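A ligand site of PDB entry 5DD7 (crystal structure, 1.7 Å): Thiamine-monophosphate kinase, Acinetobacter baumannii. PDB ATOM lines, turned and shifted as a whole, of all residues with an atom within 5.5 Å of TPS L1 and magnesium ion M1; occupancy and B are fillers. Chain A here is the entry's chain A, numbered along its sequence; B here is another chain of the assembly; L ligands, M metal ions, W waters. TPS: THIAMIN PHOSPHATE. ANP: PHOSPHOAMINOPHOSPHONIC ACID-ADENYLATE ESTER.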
ATOM      1  N   ASP A  51      24.605 -15.470 -19.557  1.00  0.00           N
ATOM      2  CA  ASP A  51      23.463 -14.958 -20.297  1.00  0.00           C
ATOM      3  C   ASP A  51      23.911 -14.560 -21.696  1.00  0.00           C
ATOM      4  O   ASP A  51      24.978 -13.962 -21.857  1.00  0.00           O
ATOM      5  CB  ASP A  51      22.836 -13.716 -19.616  1.00  0.00           C
ATOM      6  CG  ASP A  51      21.661 -14.056 -18.695  1.00  0.00           C
ATOM      7  OD1 ASP A  51      20.880 -14.973 -19.027  1.00  0.00           O
ATOM      8  OD2 ASP A  51      21.501 -13.395 -17.655  1.00  0.00           O
ATOM      9  N   THR A  52      23.076 -14.883 -22.690  1.00  0.00           N
ATOM     10  CA  THR A  52      23.338 -14.632 -24.107  1.00  0.00           C
ATOM     11  C   THR A  52      22.574 -13.403 -24.585  1.00  0.00           C
ATOM     12  O   THR A  52      21.440 -13.167 -24.160  1.00  0.00           O
ATOM     13  CB  THR A  52      22.892 -15.839 -24.937  1.00  0.00           C
ATOM     14  OG1 THR A  52      23.600 -17.008 -24.511  1.00  0.00           O
ATOM     15  CG2 THR A  52      23.075 -15.601 -26.444  1.00  0.00           C
ATOM     16  N   GLY A  56      19.367  -7.769 -32.412  1.00  0.00           N
ATOM     17  CA  GLY A  56      18.012  -7.639 -32.898  1.00  0.00           C
ATOM     18  C   GLY A  56      16.973  -8.260 -32.013  1.00  0.00           C
ATOM     19  O   GLY A  56      15.768  -8.011 -32.207  1.00  0.00           O
ATOM     20  N   ARG A  57      17.376  -9.088 -31.048  1.00  0.00           N
ATOM     21  CA  ARG A  57      16.454  -9.635 -30.066  1.00  0.00           C
ATOM     22  C   ARG A  57      16.684  -9.045 -28.685  1.00  0.00           C
ATOM     23  O   ARG A  57      15.742  -8.567 -28.060  1.00  0.00           O
ATOM     24  CB  ARG A  57      16.537 -11.168 -29.992  1.00  0.00           C
ATOM     25  CG  ARG A  57      15.470 -11.713 -29.058  1.00  0.00           C
ATOM     26  CD  ARG A  57      15.043 -13.128 -29.387  1.00  0.00           C
ATOM     27  NE  ARG A  57      14.497 -13.244 -30.726  1.00  0.00           N
ATOM     28  CZ  ARG A  57      13.198 -13.158 -31.023  1.00  0.00           C
ATOM     29  NH1 ARG A  57      12.789 -13.287 -32.279  1.00  0.00           N
ATOM     30  NH2 ARG A  57      12.311 -12.944 -30.055  1.00  0.00           N
ATOM     31  N   HIS A  58      17.936  -9.042 -28.218  1.00  0.00           N
ATOM     32  CA  HIS A  58      18.270  -8.439 -26.934  1.00  0.00           C
ATOM     33  C   HIS A  58      18.661  -6.975 -27.044  1.00  0.00           C
ATOM     34  O   HIS A  58      18.794  -6.296 -26.012  1.00  0.00           O
ATOM     35  CB  HIS A  58      19.406  -9.214 -26.255  1.00  0.00           C
ATOM     36  CG  HIS A  58      19.003 -10.597 -25.870  1.00  0.00           C
ATOM     37  ND1 HIS A  58      18.987 -11.640 -26.770  1.00  0.00           N
ATOM     38  CD2 HIS A  58      18.537 -11.093 -24.704  1.00  0.00           C
ATOM     39  CE1 HIS A  58      18.565 -12.730 -26.151  1.00  0.00           C
ATOM     40  NE2 HIS A  58      18.269 -12.416 -24.904  1.00  0.00           N
ATOM     41  N   PHE A  59      18.850  -6.465 -28.256  1.00  0.00           N
ATOM     42  CA  PHE A  59      19.116  -5.045 -28.421  1.00  0.00           C
ATOM     43  C   PHE A  59      18.749  -4.671 -29.846  1.00  0.00           C
ATOM     44  O   PHE A  59      18.869  -5.500 -30.749  1.00  0.00           O
ATOM     45  CB  PHE A  59      20.576  -4.677 -28.111  1.00  0.00           C
ATOM     46  CG  PHE A  59      21.608  -5.559 -28.767  1.00  0.00           C
ATOM     47  CD1 PHE A  59      22.045  -5.294 -30.056  1.00  0.00           C
ATOM     48  CD2 PHE A  59      22.198  -6.608 -28.070  1.00  0.00           C
ATOM     49  CE1 PHE A  59      23.033  -6.087 -30.654  1.00  0.00           C
ATOM     50  CE2 PHE A  59      23.168  -7.398 -28.660  1.00  0.00           C
ATOM     51  CZ  PHE A  59      23.606  -7.132 -29.948  1.00  0.00           C
ATOM     52  N   PRO A  60      18.275  -3.448 -30.061  1.00  0.00           N
ATOM     53  CA  PRO A  60      18.033  -2.977 -31.431  1.00  0.00           C
ATOM     54  C   PRO A  60      19.281  -3.139 -32.298  1.00  0.00           C
ATOM     55  O   PRO A  60      20.402  -2.999 -31.813  1.00  0.00           O
ATOM     56  CB  PRO A  60      17.660  -1.508 -31.230  1.00  0.00           C
ATOM     57  CG  PRO A  60      17.009  -1.485 -29.882  1.00  0.00           C
ATOM     58  CD  PRO A  60      17.820  -2.469 -29.054  1.00  0.00           C
ATOM     59  N   LYS A  71      26.222  -3.598 -21.977  1.00  0.00           N
ATOM     60  CA  LYS A  71      25.090  -4.404 -21.521  1.00  0.00           C
ATOM     61  C   LYS A  71      25.431  -5.888 -21.469  1.00  0.00           C
ATOM     62  O   LYS A  71      24.939  -6.611 -20.570  1.00  0.00           O
ATOM     63  CB  LYS A  71      23.878  -4.158 -22.430  1.00  0.00           C
ATOM     64  CG  LYS A  71      22.585  -4.812 -21.931  1.00  0.00           C
ATOM     65  CD  LYS A  71      21.344  -4.162 -22.536  1.00  0.00           C
ATOM     66  CE  LYS A  71      20.083  -4.848 -22.001  1.00  0.00           C
ATOM     67  NZ  LYS A  71      18.807  -4.185 -22.423  1.00  0.00           N
ATOM     68  N   LEU A 173      12.566   1.395 -25.190  1.00  0.00           N
ATOM     69  CA  LEU A 173      12.602   0.542 -26.382  1.00  0.00           C
ATOM     70  C   LEU A 173      11.529   0.947 -27.383  1.00  0.00           C
ATOM     71  O   LEU A 173      11.761   0.885 -28.597  1.00  0.00           O
ATOM     72  CB  LEU A 173      12.429  -0.914 -25.976  1.00  0.00           C
ATOM     73  CG  LEU A 173      12.261  -1.904 -27.132  1.00  0.00           C
ATOM     74  CD1 LEU A 173      13.510  -1.940 -28.007  1.00  0.00           C
ATOM     75  CD2 LEU A 173      11.999  -3.283 -26.519  1.00  0.00           C
ATOM     76  N   LEU A 184      17.560   1.476 -21.445  1.00  0.00           N
ATOM     77  CA  LEU A 184      17.611   0.295 -22.280  1.00  0.00           C
ATOM     78  C   LEU A 184      19.047  -0.068 -22.626  1.00  0.00           C
ATOM     79  O   LEU A 184      19.462  -1.226 -22.495  1.00  0.00           O
ATOM     80  CB  LEU A 184      16.814   0.550 -23.560  1.00  0.00           C
ATOM     81  CG  LEU A 184      16.853  -0.567 -24.598  1.00  0.00           C
ATOM     82  CD1 LEU A 184      15.998  -1.720 -24.086  1.00  0.00           C
ATOM     83  CD2 LEU A 184      16.353  -0.041 -25.947  1.00  0.00           C
ATOM     84  N   SER A 208      15.029  -8.913 -15.008  1.00  0.00           N
ATOM     85  CA  SER A 208      15.396  -8.930 -16.412  1.00  0.00           C
ATOM     86  C   SER A 208      14.192  -9.060 -17.323  1.00  0.00           C
ATOM     87  O   SER A 208      14.210  -8.535 -18.449  1.00  0.00           O
ATOM     88  CB  SER A 208      16.358 -10.090 -16.677  1.00  0.00           C
ATOM     89  OG  SER A 208      15.863 -11.284 -16.071  1.00  0.00           O
ATOM     90  N   ASP A 209      13.148  -9.762 -16.894  1.00  0.00           N
ATOM     91  CA  ASP A 209      12.017 -10.082 -17.753  1.00  0.00           C
ATOM     92  C   ASP A 209      10.766  -9.287 -17.430  1.00  0.00           C
ATOM     93  O   ASP A 209       9.850  -9.230 -18.269  1.00  0.00           O
ATOM     94  CB  ASP A 209      11.683 -11.579 -17.674  1.00  0.00           C
ATOM     95  CG  ASP A 209      12.808 -12.456 -18.203  1.00  0.00           C
ATOM     96  OD1 ASP A 209      13.459 -12.038 -19.175  1.00  0.00           O
ATOM     97  OD2 ASP A 209      13.034 -13.554 -17.638  1.00  0.00           O
ATOM     98  N   GLY A 254       7.501  -4.937 -18.563  1.00  0.00           N
ATOM     99  CA  GLY A 254       8.398  -4.433 -19.577  1.00  0.00           C
ATOM    100  C   GLY A 254       9.712  -5.183 -19.664  1.00  0.00           C
ATOM    101  O   GLY A 254      10.220  -5.462 -20.762  1.00  0.00           O
ATOM    102  N   GLY A 255      10.295  -5.514 -18.519  1.00  0.00           N
ATOM    103  CA  GLY A 255      11.610  -6.159 -18.507  1.00  0.00           C
ATOM    104  C   GLY A 255      12.733  -5.177 -18.824  1.00  0.00           C
ATOM    105  O   GLY A 255      12.540  -3.969 -19.006  1.00  0.00           O
ATOM    106  N   ASP A 256      13.952  -5.739 -18.888  1.00  0.00           N
ATOM    107  CA  ASP A 256      15.168  -4.974 -19.144  1.00  0.00           C
ATOM    108  C   ASP A 256      15.497  -3.978 -18.055  1.00  0.00           C
ATOM    109  O   ASP A 256      16.312  -3.081 -18.270  1.00  0.00           O
ATOM    110  CB  ASP A 256      15.109  -4.211 -20.477  1.00  0.00           C
ATOM    111  CG  ASP A 256      15.589  -5.046 -21.664  1.00  0.00           C
ATOM    112  OD1 ASP A 256      16.572  -5.792 -21.523  1.00  0.00           O
ATOM    113  OD2 ASP A 256      14.969  -4.918 -22.746  1.00  0.00           O
ATOM    114  N   TYR A 258      16.842  -4.614 -14.886  1.00  0.00           N
ATOM    115  CA  TYR A 258      18.049  -5.007 -14.160  1.00  0.00           C
ATOM    116  C   TYR A 258      18.153  -4.287 -12.822  1.00  0.00           C
ATOM    117  O   TYR A 258      19.237  -3.951 -12.337  1.00  0.00           O
ATOM    118  CB  TYR A 258      19.302  -4.817 -15.034  1.00  0.00           C
ATOM    119  CG  TYR A 258      19.148  -5.756 -16.209  1.00  0.00           C
ATOM    120  CD1 TYR A 258      19.340  -7.129 -16.049  1.00  0.00           C
ATOM    121  CD2 TYR A 258      18.709  -5.298 -17.443  1.00  0.00           C
ATOM    122  CE1 TYR A 258      19.137  -8.025 -17.106  1.00  0.00           C
ATOM    123  CE2 TYR A 258      18.496  -6.182 -18.504  1.00  0.00           C
ATOM    124  CZ  TYR A 258      18.718  -7.542 -18.332  1.00  0.00           C
ATOM    125  OH  TYR A 258      18.535  -8.414 -19.381  1.00  0.00           O
ATOM    126  N   TYR A 309       8.629 -11.081 -20.151  1.00  0.00           N
ATOM    127  CA  TYR A 309       9.311 -11.541 -21.348  1.00  0.00           C
ATOM    128  C   TYR A 309       9.685 -13.011 -21.208  1.00  0.00           C
ATOM    129  O   TYR A 309      10.272 -13.435 -20.205  1.00  0.00           O
ATOM    130  CB  TYR A 309      10.574 -10.705 -21.610  1.00  0.00           C
ATOM    131  CG  TYR A 309      11.190 -10.946 -22.977  1.00  0.00           C
ATOM    132  CD1 TYR A 309      12.017 -12.033 -23.203  1.00  0.00           C
ATOM    133  CD2 TYR A 309      10.947 -10.068 -24.032  1.00  0.00           C
ATOM    134  CE1 TYR A 309      12.581 -12.261 -24.446  1.00  0.00           C
ATOM    135  CE2 TYR A 309      11.519 -10.287 -25.288  1.00  0.00           C
ATOM    136  CZ  TYR A 309      12.341 -11.387 -25.470  1.00  0.00           C
ATOM    137  OH  TYR A 309      12.922 -11.621 -26.700  1.00  0.00           O
ATOM    138  N   HIS A 311      11.037 -16.251 -23.967  1.00  0.00           N
ATOM    139  CA  HIS A 311      11.307 -16.714 -25.322  1.00  0.00           C
ATOM    140  C   HIS A 311      10.317 -17.786 -25.741  1.00  0.00           C
ATOM    141  O   HIS A 311       9.835 -18.587 -24.929  1.00  0.00           O
ATOM    142  CB  HIS A 311      12.737 -17.221 -25.441  1.00  0.00           C
ATOM    143  CG  HIS A 311      13.766 -16.158 -25.249  1.00  0.00           C
ATOM    144  ND1 HIS A 311      14.117 -15.284 -26.257  1.00  0.00           N
ATOM    145  CD2 HIS A 311      14.477 -15.782 -24.159  1.00  0.00           C
ATOM    146  CE1 HIS A 311      15.033 -14.435 -25.796  1.00  0.00           C
ATOM    147  NE2 HIS A 311      15.259 -14.716 -24.525  1.00  0.00           N
ATOM    148  N   GLU B  11       9.994 -20.930 -22.955  1.00  0.00           N
ATOM    149  CA  GLU B  11      11.359 -20.981 -22.436  1.00  0.00           C
ATOM    150  C   GLU B  11      11.470 -21.765 -21.129  1.00  0.00           C
ATOM    151  O   GLU B  11      12.311 -22.660 -21.002  1.00  0.00           O
ATOM    152  CB  GLU B  11      11.858 -19.554 -22.223  1.00  0.00           C
ATOM    153  CG  GLU B  11      13.243 -19.412 -21.607  1.00  0.00           C
ATOM    154  CD  GLU B  11      13.551 -17.982 -21.226  1.00  0.00           C
ATOM    155  OE1 GLU B  11      12.747 -17.085 -21.588  1.00  0.00           O
ATOM    156  OE2 GLU B  11      14.583 -17.753 -20.564  1.00  0.00           O
ATOM    157  N   PHE B  12      10.659 -21.418 -20.133  1.00  0.00           N
ATOM    158  CA  PHE B  12      10.872 -22.022 -18.811  1.00  0.00           C
ATOM    159  C   PHE B  12      10.455 -23.492 -18.802  1.00  0.00           C
ATOM    160  O   PHE B  12      11.119 -24.306 -18.153  1.00  0.00           O
ATOM    161  CB  PHE B  12      10.135 -21.213 -17.752  1.00  0.00           C
ATOM    162  CG  PHE B  12      10.642 -19.788 -17.643  1.00  0.00           C
ATOM    163  CD1 PHE B  12      11.991 -19.544 -17.466  1.00  0.00           C
ATOM    164  CD2 PHE B  12       9.771 -18.720 -17.767  1.00  0.00           C
ATOM    165  CE1 PHE B  12      12.484 -18.247 -17.399  1.00  0.00           C
ATOM    166  CE2 PHE B  12      10.247 -17.419 -17.692  1.00  0.00           C
ATOM    167  CZ  PHE B  12      11.609 -17.179 -17.509  1.00  0.00           C
ATOM    168  N   ASP B 126      21.565 -20.611 -20.017  1.00  0.00           N
ATOM    169  CA  ASP B 126      20.648 -19.598 -20.530  1.00  0.00           C
ATOM    170  C   ASP B 126      20.013 -20.145 -21.786  1.00  0.00           C
ATOM    171  O   ASP B 126      20.669 -20.835 -22.566  1.00  0.00           O
ATOM    172  CB  ASP B 126      21.373 -18.284 -20.844  1.00  0.00           C
ATOM    173  CG  ASP B 126      20.389 -17.134 -21.080  1.00  0.00           C
ATOM    174  OD1 ASP B 126      19.413 -16.972 -20.306  1.00  0.00           O
ATOM    175  OD2 ASP B 126      20.624 -16.360 -22.026  1.00  0.00           O
ATOM    176  N   THR B 127      18.742 -19.815 -21.991  1.00  0.00           N
ATOM    177  CA  THR B 127      17.991 -20.279 -23.149  1.00  0.00           C
ATOM    178  C   THR B 127      17.418 -19.058 -23.841  1.00  0.00           C
ATOM    179  O   THR B 127      16.748 -18.248 -23.197  1.00  0.00           O
ATOM    180  CB  THR B 127      16.891 -21.246 -22.717  1.00  0.00           C
ATOM    181  OG1 THR B 127      17.478 -22.320 -21.968  1.00  0.00           O
ATOM    182  CG2 THR B 127      16.138 -21.797 -23.936  1.00  0.00           C
ATOM    183  N   THR B 128      17.698 -18.917 -25.144  1.00  0.00           N
ATOM    184  CA  THR B 128      17.189 -17.799 -25.917  1.00  0.00           C
ATOM    185  C   THR B 128      16.671 -18.285 -27.266  1.00  0.00           C
ATOM    186  O   THR B 128      17.065 -19.348 -27.758  1.00  0.00           O
ATOM    187  CB  THR B 128      18.265 -16.726 -26.185  1.00  0.00           C
ATOM    188  OG1 THR B 128      19.412 -17.321 -26.799  1.00  0.00           O
ATOM    189  CG2 THR B 128      18.723 -16.086 -24.868  1.00  0.00           C
HETATM  190  CM2 TPS L   1      15.176  -5.290 -30.015  1.00  0.00           C
HETATM  191  N3  TPS L   1      14.007  -7.856 -24.262  1.00  0.00           N
HETATM  192  C2  TPS L   1      14.772  -8.653 -24.977  1.00  0.00           C
HETATM  193  S1  TPS L   1      15.300  -9.982 -24.112  1.00  0.00           S
HETATM  194  C5  TPS L   1      14.450  -9.447 -22.685  1.00  0.00           C
HETATM  195  C4  TPS L   1      13.788  -8.294 -22.957  1.00  0.00           C
HETATM  196  CM4 TPS L   1      12.912  -7.519 -22.035  1.00  0.00           C
HETATM  197  C6  TPS L   1      14.522 -10.200 -21.379  1.00  0.00           C
HETATM  198  C7  TPS L   1      15.939 -10.590 -21.049  1.00  0.00           C
HETATM  199  O7  TPS L   1      16.408 -11.544 -22.036  1.00  0.00           O
HETATM  200  N1A TPS L   1      13.493  -6.233 -28.550  1.00  0.00           N
HETATM  201  C2A TPS L   1      14.675  -5.609 -28.645  1.00  0.00           C
HETATM  202  N3A TPS L   1      15.466  -5.258 -27.615  1.00  0.00           N
HETATM  203  C4A TPS L   1      15.043  -5.564 -26.373  1.00  0.00           C
HETATM  204  N4A TPS L   1      15.808  -5.153 -25.354  1.00  0.00           N
HETATM  205  C5A TPS L   1      13.819  -6.260 -26.166  1.00  0.00           C
HETATM  206  C6A TPS L   1      13.102  -6.558 -27.304  1.00  0.00           C
HETATM  207  C7A TPS L   1      13.340  -6.637 -24.794  1.00  0.00           C
HETATM  208  P1  TPS L   1      16.803 -13.023 -21.630  1.00  0.00           P
HETATM  209  O1  TPS L   1      18.058 -12.947 -20.729  1.00  0.00           O
HETATM  210  O2  TPS L   1      17.122 -13.751 -22.949  1.00  0.00           O
HETATM  211  O3  TPS L   1      15.672 -13.665 -20.932  1.00  0.00           O
HETATM  212  PG  ANP L   2      17.319 -13.828 -17.673  1.00  0.00           P
HETATM  213  O1G ANP L   2      18.399 -12.740 -17.454  1.00  0.00           O
HETATM  214  O2G ANP L   2      17.779 -14.812 -18.640  1.00  0.00           O
HETATM  215  O3G ANP L   2      15.984 -13.146 -18.133  1.00  0.00           O
HETATM  216  PB  ANP L   2      18.133 -15.398 -15.354  1.00  0.00           P
HETATM  217  O1B ANP L   2      18.187 -14.982 -13.957  1.00  0.00           O
HETATM  218  O2B ANP L   2      19.450 -15.201 -16.144  1.00  0.00           O
HETATM  219  N3B ANP L   2      17.019 -14.569 -16.230  1.00  0.00           N
HETATM  220  PA  ANP L   2      17.180 -17.774 -16.584  1.00  0.00           P
HETATM  221  O1A ANP L   2      18.006 -17.540 -17.843  1.00  0.00           O
HETATM  222  O2A ANP L   2      15.748 -17.404 -16.767  1.00  0.00           O
HETATM  223  O3A ANP L   2      17.788 -16.935 -15.378  1.00  0.00           O
HETATM  224  O5' ANP L   2      17.299 -19.264 -16.185  1.00  0.00           O
HETATM  225  C5' ANP L   2      16.524 -19.877 -15.123  1.00  0.00           C
HETATM  226  C4' ANP L   2      17.373 -20.955 -14.507  1.00  0.00           C
HETATM  227  O4' ANP L   2      17.585 -22.021 -15.464  1.00  0.00           O
HETATM  228  C3' ANP L   2      18.765 -20.497 -14.072  1.00  0.00           C
HETATM  229  O3' ANP L   2      19.152 -21.216 -12.902  1.00  0.00           O
HETATM  230  C2' ANP L   2      19.634 -20.861 -15.273  1.00  0.00           C
HETATM  231  O2' ANP L   2      20.971 -21.091 -14.877  1.00  0.00           O
HETATM  232  C1' ANP L   2      18.962 -22.156 -15.750  1.00  0.00           C
HETATM  233  N9  ANP L   2      19.086 -22.397 -17.186  1.00  0.00           N
HETATM  234  C8  ANP L   2      18.551 -21.654 -18.201  1.00  0.00           C
HETATM  235  N7  ANP L   2      18.728 -22.170 -19.395  1.00  0.00           N
HETATM  236  C5  ANP L   2      19.434 -23.332 -19.144  1.00  0.00           C
HETATM  237  C6  ANP L   2      19.921 -24.356 -19.987  1.00  0.00           C
HETATM  238  N6  ANP L   2      19.716 -24.387 -21.309  1.00  0.00           N
HETATM  239  N1  ANP L   2      20.591 -25.383 -19.418  1.00  0.00           N
HETATM  240  C2  ANP L   2      20.744 -25.391 -18.093  1.00  0.00           C
HETATM  241  N3  ANP L   2      20.326 -24.484 -17.192  1.00  0.00           N
HETATM  242  C4  ANP L   2      19.673 -23.480 -17.785  1.00  0.00           C
HETATM  243 MG    MG M   1      14.508 -13.899 -19.287  1.00  0.00          MG
HETATM  244 MG    MG M   2      19.413 -16.138 -18.349  1.00  0.00          MG
HETATM  245 MG    MG M   3      20.035 -13.013 -16.321  1.00  0.00          MG
HETATM  246  O   HOH W   1      11.738  -5.778 -30.413  1.00  0.00           O
HETATM  247  O   HOH W   2       9.965  -6.561 -24.619  1.00  0.00           O
HETATM  248  O   HOH W   3      17.563  -7.387 -23.554  1.00  0.00           O
HETATM  249  O   HOH W   4      13.050  -9.627 -28.302  1.00  0.00           O
HETATM  250  O   HOH W   5      19.989 -13.787 -22.131  1.00  0.00           O
HETATM  251  O   HOH W   6      12.863 -14.648 -20.447  1.00  0.00           O
HETATM  252  O   HOH W   7      14.819 -15.894 -18.796  1.00  0.00           O
HETATM  253  O   HOH W   8      19.489 -10.859 -19.086  1.00  0.00           O
HETATM  254  O   HOH W   9      18.596  -3.746 -25.092  1.00  0.00           O
HETATM  255  O   HOH W  10      20.596 -11.009 -21.569  1.00  0.00           O
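Magnesium ion M1 is bound by O3G of ANP L2 (2.0 Å). O3 of TPS L1 binds magnesium ion M1 (2.0 Å). Water W7 is bound to magnesium ion M1 (2.1 Å). OD1 of Asp 209 is bound to magnesium ion M1 (2.1 Å). Magnesium ion M1 is bound by water W6 (2.1 Å). Magnesium ion M1 is bound by the side-chain carboxylate (OD2) of Asp 209 (2.2 Å). Magnesium ion M1 has six donor atoms within binding distance.
The backbone carbonyl oxygen (O) of His 58 sits at hydrogen-bond distance from a nitrogen (N4A) of TPS L1, 3.3 Å away. The side-chain hydroxyl (OG) of Ser 208 lies within hydrogen-bond range of a nitrogen (N3B) of ANP L2 (3.5 Å). NE2 of His 311 lies within hydrogen-bond range of O2 of TPS L1. OG1 of Thr 127 of chain B is in hydrogen-bond range of N7 of ANP L2 (2.9 Å). The backbone NH of Asp 126 of chain B sits at hydrogen-bond distance from a nitrogen (N7) of ANP L2, at 3.3 Å. NE2 of His 58 is in hydrogen-bond range of O2 of TPS L1 (2.6 Å). The side-chain carboxylate of Asp 256 sits at hydrogen-bond distance from a nitrogen (N4A) of TPS L1.
O of Leu 184 sits at hydrogen-bond distance from NZ of Lys 71 (3.0 Å). The backbone NH (N) of Asp 256 sits at hydrogen-bond distance from the backbone carbonyl oxygen (O) of Ser 208 (2.8 Å). NE2 of His 58 sits at hydrogen-bond distance from O of Thr 52, 3.3 Å away. O of Asp 209 sits at hydrogen-bond distance from N of Tyr 309, 2.9 Å away. N of His 311 is in hydrogen-bond range of OE1 of Glu 11 of chain B. The side-chain carboxylate of Asp 256 is in salt-bridge range of the side-chain amino group of Lys 71 (2.9 Å).
Water W7 lies within hydrogen-bond range of OE2 of Glu 11 of chain B (2.6 Å) and O2A of ANP L2 (2.7 Å). Water W5 lies within hydrogen-bond range of O1 of TPS L1, O of Thr 52 and OD2 of Asp 126 of chain B. Water W8 lies within hydrogen-bond range of the side-chain hydroxyl of Tyr 258 and an oxygen (O1) of TPS L1. Water W9 lies within hydrogen-bond range of NZ of Lys 71 (2.7 Å), O of His 58 (2.7 Å) and N4A of TPS L1 (3.1 Å). Water W10 bridges O1 of TPS L1 and O of Thr 52. Water W3 lies within hydrogen-bond range of OD1 of Asp 256 (2.8 Å), O of His 58 (3.0 Å) and N4A of TPS L1 (3.4 Å).
The backbone carbonyl oxygen of Arg 57 lies close to a nitrogen (N1A) of TPS L1, 3.3 Å away. OD1 of Asp 51 touches O1 of TPS L1, 3.9 Å away. Gly 56 touches TPS L1 (O to CM2, 3.5 Å). Phe 59 touches TPS L1 (C to CM2, 3.6 Å). Pro 60 touches TPS L1. Leu 173 touches TPS L1. CD1 of Leu 184 touches N4A of TPS L1 (3.7 Å). Ser 208 touches TPS L1 (O to C6, 3.4 Å). Gly 254 touches TPS L1. Gly 255 touches TPS L1. Tyr 258 touches TPS L1 (OH to C7, 3.8 Å). CD2 of Tyr 309 touches C4 of TPS L1, 3.5 Å away. Thr 128 of chain B touches TPS L1 (CG2 to O2, 3.4 Å). Hydrophobic or aromatic side chains within 4 Å of TPS L1: His 58, Pro 60, Leu 173, Leu 184, Tyr 309 and His 311. Of the 23 residues printed, 17 come within 4 Å of TPS L1. The nearest printed residue that does not touch TPS L1 is Glu 11 of chain B (4.2 Å).
The nearest printed residue that does not touch magnesium ion M1 is Glu 11 of chain B (4.1 Å).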
